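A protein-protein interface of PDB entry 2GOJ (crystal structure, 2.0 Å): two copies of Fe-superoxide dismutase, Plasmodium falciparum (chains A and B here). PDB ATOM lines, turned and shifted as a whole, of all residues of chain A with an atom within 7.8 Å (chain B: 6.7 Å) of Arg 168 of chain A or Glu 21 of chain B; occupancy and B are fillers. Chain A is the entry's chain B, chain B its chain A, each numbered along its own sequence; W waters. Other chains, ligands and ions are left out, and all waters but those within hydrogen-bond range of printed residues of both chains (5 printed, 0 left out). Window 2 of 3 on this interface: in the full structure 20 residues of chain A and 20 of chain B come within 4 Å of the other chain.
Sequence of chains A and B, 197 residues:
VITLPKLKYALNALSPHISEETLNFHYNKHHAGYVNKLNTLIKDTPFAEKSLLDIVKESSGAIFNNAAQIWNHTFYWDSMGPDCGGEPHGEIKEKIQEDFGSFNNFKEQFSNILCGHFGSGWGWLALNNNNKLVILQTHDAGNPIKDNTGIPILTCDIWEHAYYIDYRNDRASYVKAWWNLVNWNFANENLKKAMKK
Of the 16 printed residues of chain B, 7 touch a printed residue of chain A. Printed residues of chain B that touch a printed residue of chain A: Glu 21, Phe 25, Lys 29, His 30, Tyr 164, Ile 165 and Arg 168. Of the 15 printed residues of chain A, 7 touch a printed residue of chain B. Printed residues of chain A that touch a printed residue of chain B: Glu 21, Glu 160, His 161, Tyr 164, Ile 165, Arg 168 and Asn 169. Hydrophobic or aromatic side chains of chain A within 4 Å of the printed part of chain B: His 161, Tyr 164 and Ile 165. Among the printed residues, 14 pairs touch across the chains.
Glu 21 of chain A touches Arg 168 of chain B, and with the chains exchanged Arg 168 of chain A touches Glu 21 of chain B. Tyr 164 of chain A touches Ile 165 of chain B, and with the chains exchanged Ile 165 of chain A touches Tyr 164 of chain B. Ile 165 of chain A touches Arg 168 of chain B, and with the chains exchanged Arg 168 of chain A touches Ile 165 of chain B. Positions printed for both chains: 21, 164, 165, 166 and 168. Of the 14 pairs that touch across the chains among the printed residues, 6 have their exchanged pair printed and touching as well.
Of the printed residues of chain B, Glu 21 of chain A touches Arg 168. Of the printed residues of chain B, Glu 160 of chain A touches His 30. Tyr 163 of chain A touches none of the printed residues of chain B. Printed residues of chain B within 4 Å of Arg 168 of chain A: Glu 21, Phe 25 and Ile 165. Glu 21 of chain B touches one residue of chain A. Of the printed residues of chain A, Tyr 164 of chain B touches His 161 and Ile 165. The nearest residue of chain A that does not touch Glu 21 of chain B is Tyr 164 of chain A (6.9 Å).
Water W4 lies within hydrogen-bond range of the side-chain amide oxygen (OD1) of Asn 169 of chain A (2.7 Å) and the side-chain amino group (NZ) of Lys 29 of chain B (2.9 Å). Water W5 lies within hydrogen-bond range of OE1 of Glu 21 of chain B (2.7 Å) and NH2 of Arg 168 of chain A (3.4 Å). Water W2 lies within hydrogen-bond range of OH of Tyr 164 of chain B (2.7 Å) and O of His 161 of chain A (2.9 Å). Water W1 lies within hydrogen-bond range of the side-chain hydroxyl (OH) of Tyr 164 of chain A (3.0 Å), the backbone NH (N) of His 26 of chain B (3.2 Å) and the backbone carbonyl oxygen (O) of Thr 22 of chain B (3.5 Å). Water W3 bridges NH1 of Arg 168 of chain B (3.3 Å) and NH2 of Arg 168 of chain A (3.4 Å).
Among the printed residues, merely in contact across the chains: Asn 169 of chain A with Lys 29 of chain B, Asn 169 of chain A with His 30 of chain B, Ile 165 of chain A with Arg 168 of chain B, Asn 169 of chain A with Phe 25 of chain B, His 161 of chain A with Tyr 164 of chain B, Arg 168 of chain A with Phe 25 of chain B, Arg 168 of chain A with Ile 165 of chain B, Ile 165 of chain A with Tyr 164 of chain B, Tyr 164 of chain A with Ile 165 of chain B, Glu 160 of chain A with His 30 of chain B and Tyr 164 of chain A with Phe 25 of chain B.
O of Ile 165 of chain B is in hydrogen-bond range of NH1 of Arg 168 of chain B. O of Tyr 164 of chain B sits at hydrogen-bond distance from NH1 of Arg 168 of chain B (3.0 Å). The backbone carbonyl oxygen (O) of Ile 165 of chain A sits at hydrogen-bond distance from the guanidinium group (NH1) of Arg 168 of chain A, 3.2 Å away. The backbone carbonyl oxygen (O) of Tyr 164 of chain A lies within hydrogen-bond range of the guanidinium group (NH1) of Arg 168 of chain A, 3.0 Å away. The backbone NH (N) of His 30 of chain B sits at hydrogen-bond distance from the backbone carbonyl oxygen (O) of Phe 25 of chain B (2.9 Å). The side-chain hydroxyl (OG) of Ser 19 of chain B lies close to the backbone NH (N) of Glu 21 of chain B (3.4 Å).
A ring nitrogen (NE2) of His 30 of chain B sits at hydrogen-bond distance from the side-chain hydroxyl of Tyr 164 of chain A (2.7 Å). The guanidinium group (NH2) of Arg 168 of chain B is in salt-bridge range of the side-chain carboxylate (OE2) of Glu 21 of chain A. NH2 of Arg 168 of chain A lies within salt-bridge range of OE2 of Glu 21 of chain B.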
ATOM      1  N   GLU A  21     -22.532  10.459  -6.082  1.00  0.00           N
ATOM      2  CA  GLU A  21     -23.069   9.151  -6.475  1.00  0.00           C
ATOM      3  C   GLU A  21     -22.069   8.403  -7.364  1.00  0.00           C
ATOM      4  O   GLU A  21     -21.812   7.211  -7.179  1.00  0.00           O
ATOM      5  CB  GLU A  21     -24.396   9.299  -7.222  1.00  0.00           C
ATOM      6  CG  GLU A  21     -25.017   7.963  -7.581  1.00  0.00           C
ATOM      7  CD  GLU A  21     -26.388   8.093  -8.213  1.00  0.00           C
ATOM      8  OE1 GLU A  21     -27.042   9.170  -8.110  1.00  0.00           O
ATOM      9  OE2 GLU A  21     -26.815   7.092  -8.810  1.00  0.00           O
ATOM     10  N   GLU A 160     -16.891   4.030 -19.421  1.00  0.00           N
ATOM     11  CA  GLU A 160     -18.175   4.709 -19.371  1.00  0.00           C
ATOM     12  C   GLU A 160     -18.712   4.858 -17.950  1.00  0.00           C
ATOM     13  O   GLU A 160     -19.378   5.846 -17.667  1.00  0.00           O
ATOM     14  CB  GLU A 160     -19.192   4.047 -20.300  1.00  0.00           C
ATOM     15  CG  GLU A 160     -18.839   4.142 -21.774  1.00  0.00           C
ATOM     16  CD  GLU A 160     -19.836   3.425 -22.679  1.00  0.00           C
ATOM     17  OE1 GLU A 160     -20.227   2.275 -22.372  1.00  0.00           O
ATOM     18  OE2 GLU A 160     -20.207   4.006 -23.717  1.00  0.00           O
ATOM     19  N   HIS A 161     -18.396   3.937 -17.040  1.00  0.00           N
ATOM     20  CA  HIS A 161     -18.890   4.053 -15.662  1.00  0.00           C
ATOM     21  C   HIS A 161     -18.333   5.296 -14.951  1.00  0.00           C
ATOM     22  O   HIS A 161     -18.929   5.763 -13.994  1.00  0.00           O
ATOM     23  CB  HIS A 161     -18.617   2.786 -14.827  1.00  0.00           C
ATOM     24  CG  HIS A 161     -17.165   2.449 -14.686  1.00  0.00           C
ATOM     25  ND1 HIS A 161     -16.603   1.330 -15.260  1.00  0.00           N
ATOM     26  CD2 HIS A 161     -16.160   3.085 -14.041  1.00  0.00           C
ATOM     27  CE1 HIS A 161     -15.312   1.294 -14.982  1.00  0.00           C
ATOM     28  NE2 HIS A 161     -15.016   2.350 -14.248  1.00  0.00           N
ATOM     29  N   ALA A 162     -17.185   5.801 -15.411  1.00  0.00           N
ATOM     30  CA  ALA A 162     -16.549   7.000 -14.843  1.00  0.00           C
ATOM     31  C   ALA A 162     -17.417   8.247 -14.950  1.00  0.00           C
ATOM     32  O   ALA A 162     -17.306   9.156 -14.129  1.00  0.00           O
ATOM     33  CB  ALA A 162     -15.215   7.260 -15.512  1.00  0.00           C
ATOM     34  N   TYR A 163     -18.289   8.258 -15.955  1.00  0.00           N
ATOM     35  CA  TYR A 163     -19.058   9.444 -16.311  1.00  0.00           C
ATOM     36  C   TYR A 163     -20.531   9.224 -16.643  1.00  0.00           C
ATOM     37  O   TYR A 163     -21.283  10.197 -16.696  1.00  0.00           O
ATOM     38  CB  TYR A 163     -18.360  10.195 -17.462  1.00  0.00           C
ATOM     39  CG  TYR A 163     -18.207   9.448 -18.790  1.00  0.00           C
ATOM     40  CD1 TYR A 163     -19.235   9.425 -19.723  1.00  0.00           C
ATOM     41  CD2 TYR A 163     -16.999   8.838 -19.135  1.00  0.00           C
ATOM     42  CE1 TYR A 163     -19.084   8.771 -20.957  1.00  0.00           C
ATOM     43  CE2 TYR A 163     -16.832   8.184 -20.373  1.00  0.00           C
ATOM     44  CZ  TYR A 163     -17.879   8.152 -21.268  1.00  0.00           C
ATOM     45  OH  TYR A 163     -17.729   7.522 -22.487  1.00  0.00           O
ATOM     46  N   TYR A 164     -20.975   7.985 -16.841  1.00  0.00           N
ATOM     47  CA  TYR A 164     -22.308   7.788 -17.416  1.00  0.00           C
ATOM     48  C   TYR A 164     -23.437   8.338 -16.522  1.00  0.00           C
ATOM     49  O   TYR A 164     -24.456   8.791 -17.027  1.00  0.00           O
ATOM     50  CB  TYR A 164     -22.575   6.314 -17.825  1.00  0.00           C
ATOM     51  CG  TYR A 164     -23.369   6.244 -19.098  1.00  0.00           C
ATOM     52  CD1 TYR A 164     -22.774   6.537 -20.326  1.00  0.00           C
ATOM     53  CD2 TYR A 164     -24.738   5.952 -19.082  1.00  0.00           C
ATOM     54  CE1 TYR A 164     -23.513   6.539 -21.498  1.00  0.00           C
ATOM     55  CE2 TYR A 164     -25.481   5.942 -20.259  1.00  0.00           C
ATOM     56  CZ  TYR A 164     -24.861   6.235 -21.460  1.00  0.00           C
ATOM     57  OH  TYR A 164     -25.577   6.230 -22.633  1.00  0.00           O
ATOM     58  N   ILE A 165     -23.264   8.287 -15.207  1.00  0.00           N
ATOM     59  CA  ILE A 165     -24.303   8.749 -14.290  1.00  0.00           C
ATOM     60  C   ILE A 165     -24.502  10.249 -14.421  1.00  0.00           C
ATOM     61  O   ILE A 165     -25.626  10.736 -14.344  1.00  0.00           O
ATOM     62  CB  ILE A 165     -23.979   8.386 -12.817  1.00  0.00           C
ATOM     63  CG1 ILE A 165     -24.009   6.864 -12.614  1.00  0.00           C
ATOM     64  CG2 ILE A 165     -24.989   9.068 -11.854  1.00  0.00           C
ATOM     65  CD1 ILE A 165     -23.338   6.374 -11.299  1.00  0.00           C
ATOM     66  N   ASP A 166     -23.416  10.981 -14.628  1.00  0.00           N
ATOM     67  CA  ASP A 166     -23.482  12.438 -14.637  1.00  0.00           C
ATOM     68  C   ASP A 166     -23.643  13.045 -16.033  1.00  0.00           C
ATOM     69  O   ASP A 166     -24.231  14.118 -16.169  1.00  0.00           O
ATOM     70  CB  ASP A 166     -22.238  13.014 -13.980  1.00  0.00           C
ATOM     71  CG  ASP A 166     -21.995  12.438 -12.601  1.00  0.00           C
ATOM     72  OD1 ASP A 166     -22.991  12.220 -11.859  1.00  0.00           O
ATOM     73  OD2 ASP A 166     -20.836  12.183 -12.194  1.00  0.00           O
ATOM     74  N   TYR A 167     -23.121  12.355 -17.051  1.00  0.00           N
ATOM     75  CA  TYR A 167     -22.974  12.919 -18.401  1.00  0.00           C
ATOM     76  C   TYR A 167     -23.553  12.032 -19.496  1.00  0.00           C
ATOM     77  O   TYR A 167     -23.651  12.456 -20.638  1.00  0.00           O
ATOM     78  CB  TYR A 167     -21.484  13.202 -18.690  1.00  0.00           C
ATOM     79  CG  TYR A 167     -20.899  14.226 -17.732  1.00  0.00           C
ATOM     80  CD1 TYR A 167     -21.204  15.576 -17.863  1.00  0.00           C
ATOM     81  CD2 TYR A 167     -20.067  13.837 -16.676  1.00  0.00           C
ATOM     82  CE1 TYR A 167     -20.684  16.523 -16.984  1.00  0.00           C
ATOM     83  CE2 TYR A 167     -19.539  14.775 -15.791  1.00  0.00           C
ATOM     84  CZ  TYR A 167     -19.857  16.118 -15.951  1.00  0.00           C
ATOM     85  OH  TYR A 167     -19.360  17.060 -15.078  1.00  0.00           O
ATOM     86  N   ARG A 168     -23.978  10.822 -19.129  1.00  0.00           N
ATOM     87  CA  ARG A 168     -24.444   9.830 -20.095  1.00  0.00           C
ATOM     88  C   ARG A 168     -23.402   9.668 -21.210  1.00  0.00           C
ATOM     89  O   ARG A 168     -22.233   9.432 -20.919  1.00  0.00           O
ATOM     90  CB  ARG A 168     -25.844  10.193 -20.612  1.00  0.00           C
ATOM     91  CG  ARG A 168     -26.903  10.298 -19.521  1.00  0.00           C
ATOM     92  CD  ARG A 168     -27.588   8.980 -19.176  1.00  0.00           C
ATOM     93  NE  ARG A 168     -28.695   9.172 -18.239  1.00  0.00           N
ATOM     94  CZ  ARG A 168     -28.586   9.154 -16.908  1.00  0.00           C
ATOM     95  NH1 ARG A 168     -27.411   8.945 -16.324  1.00  0.00           N
ATOM     96  NH2 ARG A 168     -29.662   9.344 -16.146  1.00  0.00           N
ATOM     97  N   ASN A 169     -23.813   9.792 -22.474  1.00  0.00           N
ATOM     98  CA  ASN A 169     -22.915   9.614 -23.624  1.00  0.00           C
ATOM     99  C   ASN A 169     -21.943  10.771 -23.850  1.00  0.00           C
ATOM    100  O   ASN A 169     -21.027  10.657 -24.657  1.00  0.00           O
ATOM    101  CB  ASN A 169     -23.757   9.437 -24.905  1.00  0.00           C
ATOM    102  CG  ASN A 169     -24.501  10.707 -25.287  1.00  0.00           C
ATOM    103  OD1 ASN A 169     -25.394  11.163 -24.570  1.00  0.00           O
ATOM    104  ND2 ASN A 169     -24.106  11.305 -26.392  1.00  0.00           N
ATOM    105  N   ASP A 170     -22.152  11.881 -23.143  1.00  0.00           N
ATOM    106  CA  ASP A 170     -21.394  13.116 -23.377  1.00  0.00           C
ATOM    107  C   ASP A 170     -20.018  13.098 -22.706  1.00  0.00           C
ATOM    108  O   ASP A 170     -19.783  13.785 -21.713  1.00  0.00           O
ATOM    109  CB  ASP A 170     -22.224  14.314 -22.892  1.00  0.00           C
ATOM    110  CG  ASP A 170     -21.646  15.660 -23.330  1.00  0.00           C
ATOM    111  OD1 ASP A 170     -20.640  15.696 -24.049  1.00  0.00           O
ATOM    112  OD2 ASP A 170     -22.135  16.735 -22.971  1.00  0.00           O
ATOM    113  N   ARG A 171     -19.102  12.307 -23.255  1.00  0.00           N
ATOM    114  CA  ARG A 171     -17.777  12.185 -22.674  1.00  0.00           C
ATOM    115  C   ARG A 171     -17.022  13.515 -22.731  1.00  0.00           C
ATOM    116  O   ARG A 171     -16.218  13.815 -21.847  1.00  0.00           O
ATOM    117  CB  ARG A 171     -16.969  11.108 -23.393  1.00  0.00           C
ATOM    118  CG  ARG A 171     -15.648  10.815 -22.723  1.00  0.00           C
ATOM    119  CD  ARG A 171     -14.692  10.045 -23.603  1.00  0.00           C
ATOM    120  NE  ARG A 171     -15.133   8.671 -23.793  1.00  0.00           N
ATOM    121  CZ  ARG A 171     -14.539   7.815 -24.614  1.00  0.00           C
ATOM    122  NH1 ARG A 171     -13.472   8.190 -25.310  1.00  0.00           N
ATOM    123  NH2 ARG A 171     -15.007   6.579 -24.735  1.00  0.00           N
ATOM    124  N   ALA A 172     -17.266  14.304 -23.774  1.00  0.00           N
ATOM    125  CA  ALA A 172     -16.609  15.611 -23.913  1.00  0.00           C
ATOM    126  C   ALA A 172     -16.848  16.510 -22.705  1.00  0.00           C
ATOM    127  O   ALA A 172     -15.915  17.139 -22.207  1.00  0.00           O
ATOM    128  CB  ALA A 172     -17.036  16.307 -25.198  1.00  0.00           C
ATOM    129  N   TYR A 174     -17.654  15.466 -19.678  1.00  0.00           N
ATOM    130  CA  TYR A 174     -16.910  14.869 -18.580  1.00  0.00           C
ATOM    131  C   TYR A 174     -15.447  15.278 -18.597  1.00  0.00           C
ATOM    132  O   TYR A 174     -14.893  15.643 -17.570  1.00  0.00           O
ATOM    133  CB  TYR A 174     -17.014  13.360 -18.641  1.00  0.00           C
ATOM    134  CG  TYR A 174     -15.963  12.608 -17.855  1.00  0.00           C
ATOM    135  CD1 TYR A 174     -15.971  12.603 -16.453  1.00  0.00           C
ATOM    136  CD2 TYR A 174     -14.993  11.868 -18.505  1.00  0.00           C
ATOM    137  CE1 TYR A 174     -15.033  11.869 -15.732  1.00  0.00           C
ATOM    138  CE2 TYR A 174     -14.031  11.150 -17.787  1.00  0.00           C
ATOM    139  CZ  TYR A 174     -14.062  11.143 -16.410  1.00  0.00           C
ATOM    140  OH  TYR A 174     -13.116  10.412 -15.718  1.00  0.00           O
ATOM    141  N   LEU B  11     -39.884   3.253 -28.160  1.00  0.00           N
ATOM    142  CA  LEU B  11     -38.737   3.433 -27.260  1.00  0.00           C
ATOM    143  C   LEU B  11     -38.965   2.828 -25.895  1.00  0.00           C
ATOM    144  O   LEU B  11     -38.007   2.446 -25.223  1.00  0.00           O
ATOM    145  CB  LEU B  11     -38.409   4.923 -27.057  1.00  0.00           C
ATOM    146  CG  LEU B  11     -37.548   5.703 -28.040  1.00  0.00           C
ATOM    147  CD1 LEU B  11     -37.329   7.117 -27.467  1.00  0.00           C
ATOM    148  CD2 LEU B  11     -36.211   5.056 -28.374  1.00  0.00           C
ATOM    149  N   ILE B  18     -35.345  -3.038 -20.128  1.00  0.00           N
ATOM    150  CA  ILE B  18     -34.512  -1.932 -20.558  1.00  0.00           C
ATOM    151  C   ILE B  18     -35.443  -0.718 -20.656  1.00  0.00           C
ATOM    152  O   ILE B  18     -36.461  -0.762 -21.342  1.00  0.00           O
ATOM    153  CB  ILE B  18     -33.800  -2.254 -21.900  1.00  0.00           C
ATOM    154  CG1 ILE B  18     -32.885  -3.481 -21.740  1.00  0.00           C
ATOM    155  CG2 ILE B  18     -32.969  -1.084 -22.354  1.00  0.00           C
ATOM    156  CD1 ILE B  18     -32.233  -3.924 -23.009  1.00  0.00           C
ATOM    157  N   SER B  19     -35.092   0.350 -19.946  1.00  0.00           N
ATOM    158  CA  SER B  19     -35.952   1.538 -19.842  1.00  0.00           C
ATOM    159  C   SER B  19     -36.017   2.319 -21.129  1.00  0.00           C
ATOM    160  O   SER B  19     -35.152   2.193 -22.001  1.00  0.00           O
ATOM    161  CB  SER B  19     -35.497   2.467 -18.702  1.00  0.00           C
ATOM    162  OG  SER B  19     -34.301   3.180 -19.008  1.00  0.00           O
ATOM    163  N   GLU B  20     -37.062   3.131 -21.232  1.00  0.00           N
ATOM    164  CA  GLU B  20     -37.210   4.098 -22.323  1.00  0.00           C
ATOM    165  C   GLU B  20     -36.012   5.043 -22.380  1.00  0.00           C
ATOM    166  O   GLU B  20     -35.504   5.334 -23.450  1.00  0.00           O
ATOM    167  CB  GLU B  20     -38.515   4.900 -22.163  1.00  0.00           C
ATOM    168  CG  GLU B  20     -38.870   5.721 -23.398  1.00  0.00           C
ATOM    169  CD  GLU B  20     -40.185   6.499 -23.268  1.00  0.00           C
ATOM    170  OE1 GLU B  20     -40.418   7.374 -24.114  1.00  0.00           O
ATOM    171  OE2 GLU B  20     -40.985   6.231 -22.343  1.00  0.00           O
ATOM    172  N   GLU B  21     -35.541   5.497 -21.225  1.00  0.00           N
ATOM    173  CA  GLU B  21     -34.382   6.388 -21.167  1.00  0.00           C
ATOM    174  C   GLU B  21     -33.167   5.736 -21.804  1.00  0.00           C
ATOM    175  O   GLU B  21     -32.450   6.371 -22.567  1.00  0.00           O
ATOM    176  CB  GLU B  21     -34.034   6.771 -19.716  1.00  0.00           C
ATOM    177  CG  GLU B  21     -32.852   7.721 -19.650  1.00  0.00           C
ATOM    178  CD  GLU B  21     -32.602   8.329 -18.284  1.00  0.00           C
ATOM    179  OE1 GLU B  21     -33.277   7.964 -17.299  1.00  0.00           O
ATOM    180  OE2 GLU B  21     -31.686   9.171 -18.213  1.00  0.00           O
ATOM    181  N   THR B  22     -32.926   4.470 -21.459  1.00  0.00           N
ATOM    182  CA  THR B  22     -31.774   3.750 -21.999  1.00  0.00           C
ATOM    183  C   THR B  22     -31.898   3.638 -23.507  1.00  0.00           C
ATOM    184  O   THR B  22     -30.957   3.948 -24.237  1.00  0.00           O
ATOM    185  CB  THR B  22     -31.635   2.367 -21.361  1.00  0.00           C
ATOM    186  OG1 THR B  22     -31.122   2.509 -20.029  1.00  0.00           O
ATOM    187  CG2 THR B  22     -30.583   1.526 -22.109  1.00  0.00           C
ATOM    188  N   LEU B  23     -33.071   3.230 -23.979  1.00  0.00           N
ATOM    189  CA  LEU B  23     -33.272   3.093 -25.417  1.00  0.00           C
ATOM    190  C   LEU B  23     -33.065   4.431 -26.106  1.00  0.00           C
ATOM    191  O   LEU B  23     -32.509   4.496 -27.206  1.00  0.00           O
ATOM    192  CB  LEU B  23     -34.652   2.509 -25.750  1.00  0.00           C
ATOM    193  CG  LEU B  23     -34.580   1.166 -26.481  1.00  0.00           C
ATOM    194  CD1 LEU B  23     -35.965   0.589 -26.703  1.00  0.00           C
ATOM    195  CD2 LEU B  23     -33.857   1.303 -27.845  1.00  0.00           C
ATOM    196  N   ASN B  24     -33.501   5.501 -25.453  1.00  0.00           N
ATOM    197  CA  ASN B  24     -33.378   6.841 -26.018  1.00  0.00           C
ATOM    198  C   ASN B  24     -31.899   7.209 -26.210  1.00  0.00           C
ATOM    199  O   ASN B  24     -31.486   7.608 -27.298  1.00  0.00           O
ATOM    200  CB  ASN B  24     -34.113   7.888 -25.153  1.00  0.00           C
ATOM    201  CG  ASN B  24     -34.290   9.231 -25.878  1.00  0.00           C
ATOM    202  OD1 ASN B  24     -34.186   9.309 -27.114  1.00  0.00           O
ATOM    203  ND2 ASN B  24     -34.559  10.287 -25.116  1.00  0.00           N
ATOM    204  N   PHE B  25     -31.097   7.034 -25.171  1.00  0.00           N
ATOM    205  CA  PHE B  25     -29.665   7.334 -25.267  1.00  0.00           C
ATOM    206  C   PHE B  25     -28.935   6.350 -26.176  1.00  0.00           C
ATOM    207  O   PHE B  25     -28.153   6.755 -27.022  1.00  0.00           O
ATOM    208  CB  PHE B  25     -29.023   7.387 -23.869  1.00  0.00           C
ATOM    209  CG  PHE B  25     -29.251   8.689 -23.165  1.00  0.00           C
ATOM    210  CD1 PHE B  25     -30.336   8.858 -22.309  1.00  0.00           C
ATOM    211  CD2 PHE B  25     -28.406   9.761 -23.383  1.00  0.00           C
ATOM    212  CE1 PHE B  25     -30.568  10.084 -21.670  1.00  0.00           C
ATOM    213  CE2 PHE B  25     -28.643  10.991 -22.768  1.00  0.00           C
ATOM    214  CZ  PHE B  25     -29.722  11.147 -21.901  1.00  0.00           C
ATOM    215  N   HIS B  26     -29.209   5.060 -26.006  1.00  0.00           N
ATOM    216  CA  HIS B  26     -28.503   3.998 -26.732  1.00  0.00           C
ATOM    217  C   HIS B  26     -28.785   4.086 -28.240  1.00  0.00           C
ATOM    218  O   HIS B  26     -27.878   3.952 -29.053  1.00  0.00           O
ATOM    219  CB  HIS B  26     -28.909   2.617 -26.161  1.00  0.00           C
ATOM    220  CG  HIS B  26     -27.915   1.529 -26.396  1.00  0.00           C
ATOM    221  ND1 HIS B  26     -27.990   0.311 -25.753  1.00  0.00           N
ATOM    222  CD2 HIS B  26     -26.813   1.473 -27.184  1.00  0.00           C
ATOM    223  CE1 HIS B  26     -26.968  -0.439 -26.123  1.00  0.00           C
ATOM    224  NE2 HIS B  26     -26.237   0.244 -26.989  1.00  0.00           N
ATOM    225  N   LYS B  29     -28.760   8.496 -29.454  1.00  0.00           N
ATOM    226  CA  LYS B  29     -27.450   9.127 -29.242  1.00  0.00           C
ATOM    227  C   LYS B  29     -26.282   8.248 -29.678  1.00  0.00           C
ATOM    228  O   LYS B  29     -25.558   8.618 -30.569  1.00  0.00           O
ATOM    229  CB  LYS B  29     -27.260   9.575 -27.785  1.00  0.00           C
ATOM    230  CG  LYS B  29     -28.265  10.641 -27.338  1.00  0.00           C
ATOM    231  CD  LYS B  29     -27.832  12.051 -27.744  1.00  0.00           C
ATOM    232  CE  LYS B  29     -27.422  12.903 -26.538  1.00  0.00           C
ATOM    233  NZ  LYS B  29     -28.402  12.807 -25.412  1.00  0.00           N
ATOM    234  N   HIS B  30     -26.093   7.086 -29.059  1.00  0.00           N
ATOM    235  CA  HIS B  30     -24.944   6.234 -29.395  1.00  0.00           C
ATOM    236  C   HIS B  30     -25.037   5.719 -30.834  1.00  0.00           C
ATOM    237  O   HIS B  30     -24.135   5.930 -31.649  1.00  0.00           O
ATOM    238  CB  HIS B  30     -24.819   5.040 -28.432  1.00  0.00           C
ATOM    239  CG  HIS B  30     -24.397   5.420 -27.052  1.00  0.00           C
ATOM    240  ND1 HIS B  30     -23.080   5.644 -26.713  1.00  0.00           N
ATOM    241  CD2 HIS B  30     -25.120   5.637 -25.928  1.00  0.00           C
ATOM    242  CE1 HIS B  30     -23.009   5.978 -25.437  1.00  0.00           C
ATOM    243  NE2 HIS B  30     -24.231   5.974 -24.934  1.00  0.00           N
ATOM    244  N   TYR B 164     -26.068   0.923 -17.770  1.00  0.00           N
ATOM    245  CA  TYR B 164     -25.648   1.655 -16.566  1.00  0.00           C
ATOM    246  C   TYR B 164     -26.748   2.532 -15.949  1.00  0.00           C
ATOM    247  O   TYR B 164     -26.774   2.722 -14.730  1.00  0.00           O
ATOM    248  CB  TYR B 164     -24.377   2.490 -16.798  1.00  0.00           C
ATOM    249  CG  TYR B 164     -23.480   2.485 -15.572  1.00  0.00           C
ATOM    250  CD1 TYR B 164     -22.652   1.393 -15.297  1.00  0.00           C
ATOM    251  CD2 TYR B 164     -23.487   3.546 -14.677  1.00  0.00           C
ATOM    252  CE1 TYR B 164     -21.846   1.361 -14.168  1.00  0.00           C
ATOM    253  CE2 TYR B 164     -22.677   3.535 -13.544  1.00  0.00           C
ATOM    254  CZ  TYR B 164     -21.861   2.447 -13.296  1.00  0.00           C
ATOM    255  OH  TYR B 164     -21.081   2.442 -12.179  1.00  0.00           O
ATOM    256  N   ILE B 165     -27.649   3.049 -16.785  1.00  0.00           N
ATOM    257  CA  ILE B 165     -28.779   3.864 -16.314  1.00  0.00           C
ATOM    258  C   ILE B 165     -29.725   3.048 -15.441  1.00  0.00           C
ATOM    259  O   ILE B 165     -30.200   3.537 -14.425  1.00  0.00           O
ATOM    260  CB  ILE B 165     -29.575   4.484 -17.510  1.00  0.00           C
ATOM    261  CG1 ILE B 165     -28.652   5.333 -18.397  1.00  0.00           C
ATOM    262  CG2 ILE B 165     -30.747   5.347 -16.996  1.00  0.00           C
ATOM    263  CD1 ILE B 165     -29.293   5.794 -19.651  1.00  0.00           C
ATOM    264  N   ASP B 166     -30.002   1.812 -15.850  1.00  0.00           N
ATOM    265  CA  ASP B 166     -31.025   0.982 -15.199  1.00  0.00           C
ATOM    266  C   ASP B 166     -30.450   0.094 -14.111  1.00  0.00           C
ATOM    267  O   ASP B 166     -31.143  -0.232 -13.147  1.00  0.00           O
ATOM    268  CB  ASP B 166     -31.719   0.099 -16.233  1.00  0.00           C
ATOM    269  CG  ASP B 166     -32.286   0.890 -17.380  1.00  0.00           C
ATOM    270  OD1 ASP B 166     -32.772   2.016 -17.127  1.00  0.00           O
ATOM    271  OD2 ASP B 166     -32.275   0.473 -18.560  1.00  0.00           O
ATOM    272  N   ARG B 168     -26.730   0.245 -13.175  1.00  0.00           N
ATOM    273  CA  ARG B 168     -25.400   0.671 -12.738  1.00  0.00           C
ATOM    274  C   ARG B 168     -24.384  -0.444 -13.022  1.00  0.00           C
ATOM    275  O   ARG B 168     -24.324  -0.953 -14.134  1.00  0.00           O
ATOM    276  CB  ARG B 168     -25.425   1.103 -11.258  1.00  0.00           C
ATOM    277  CG  ARG B 168     -26.317   2.311 -10.990  1.00  0.00           C
ATOM    278  CD  ARG B 168     -25.661   3.631 -11.365  1.00  0.00           C
ATOM    279  NE  ARG B 168     -26.456   4.789 -10.962  1.00  0.00           N
ATOM    280  CZ  ARG B 168     -27.432   5.331 -11.679  1.00  0.00           C
ATOM    281  NH1 ARG B 168     -27.750   4.836 -12.866  1.00  0.00           N
ATOM    282  NH2 ARG B 168     -28.092   6.381 -11.217  1.00  0.00           N
HETATM  283  O   HOH W   1     -27.589   4.174 -23.389  1.00  0.00           O
HETATM  284  O   HOH W   2     -19.382   4.449 -11.407  1.00  0.00           O
HETATM  285  O   HOH W   3     -30.073   6.983 -13.799  1.00  0.00           O
HETATM  286  O   HOH W   4     -26.167  13.608 -23.818  1.00  0.00           O
HETATM  287  O   HOH W   5     -32.456   8.123 -14.722  1.00  0.00           O
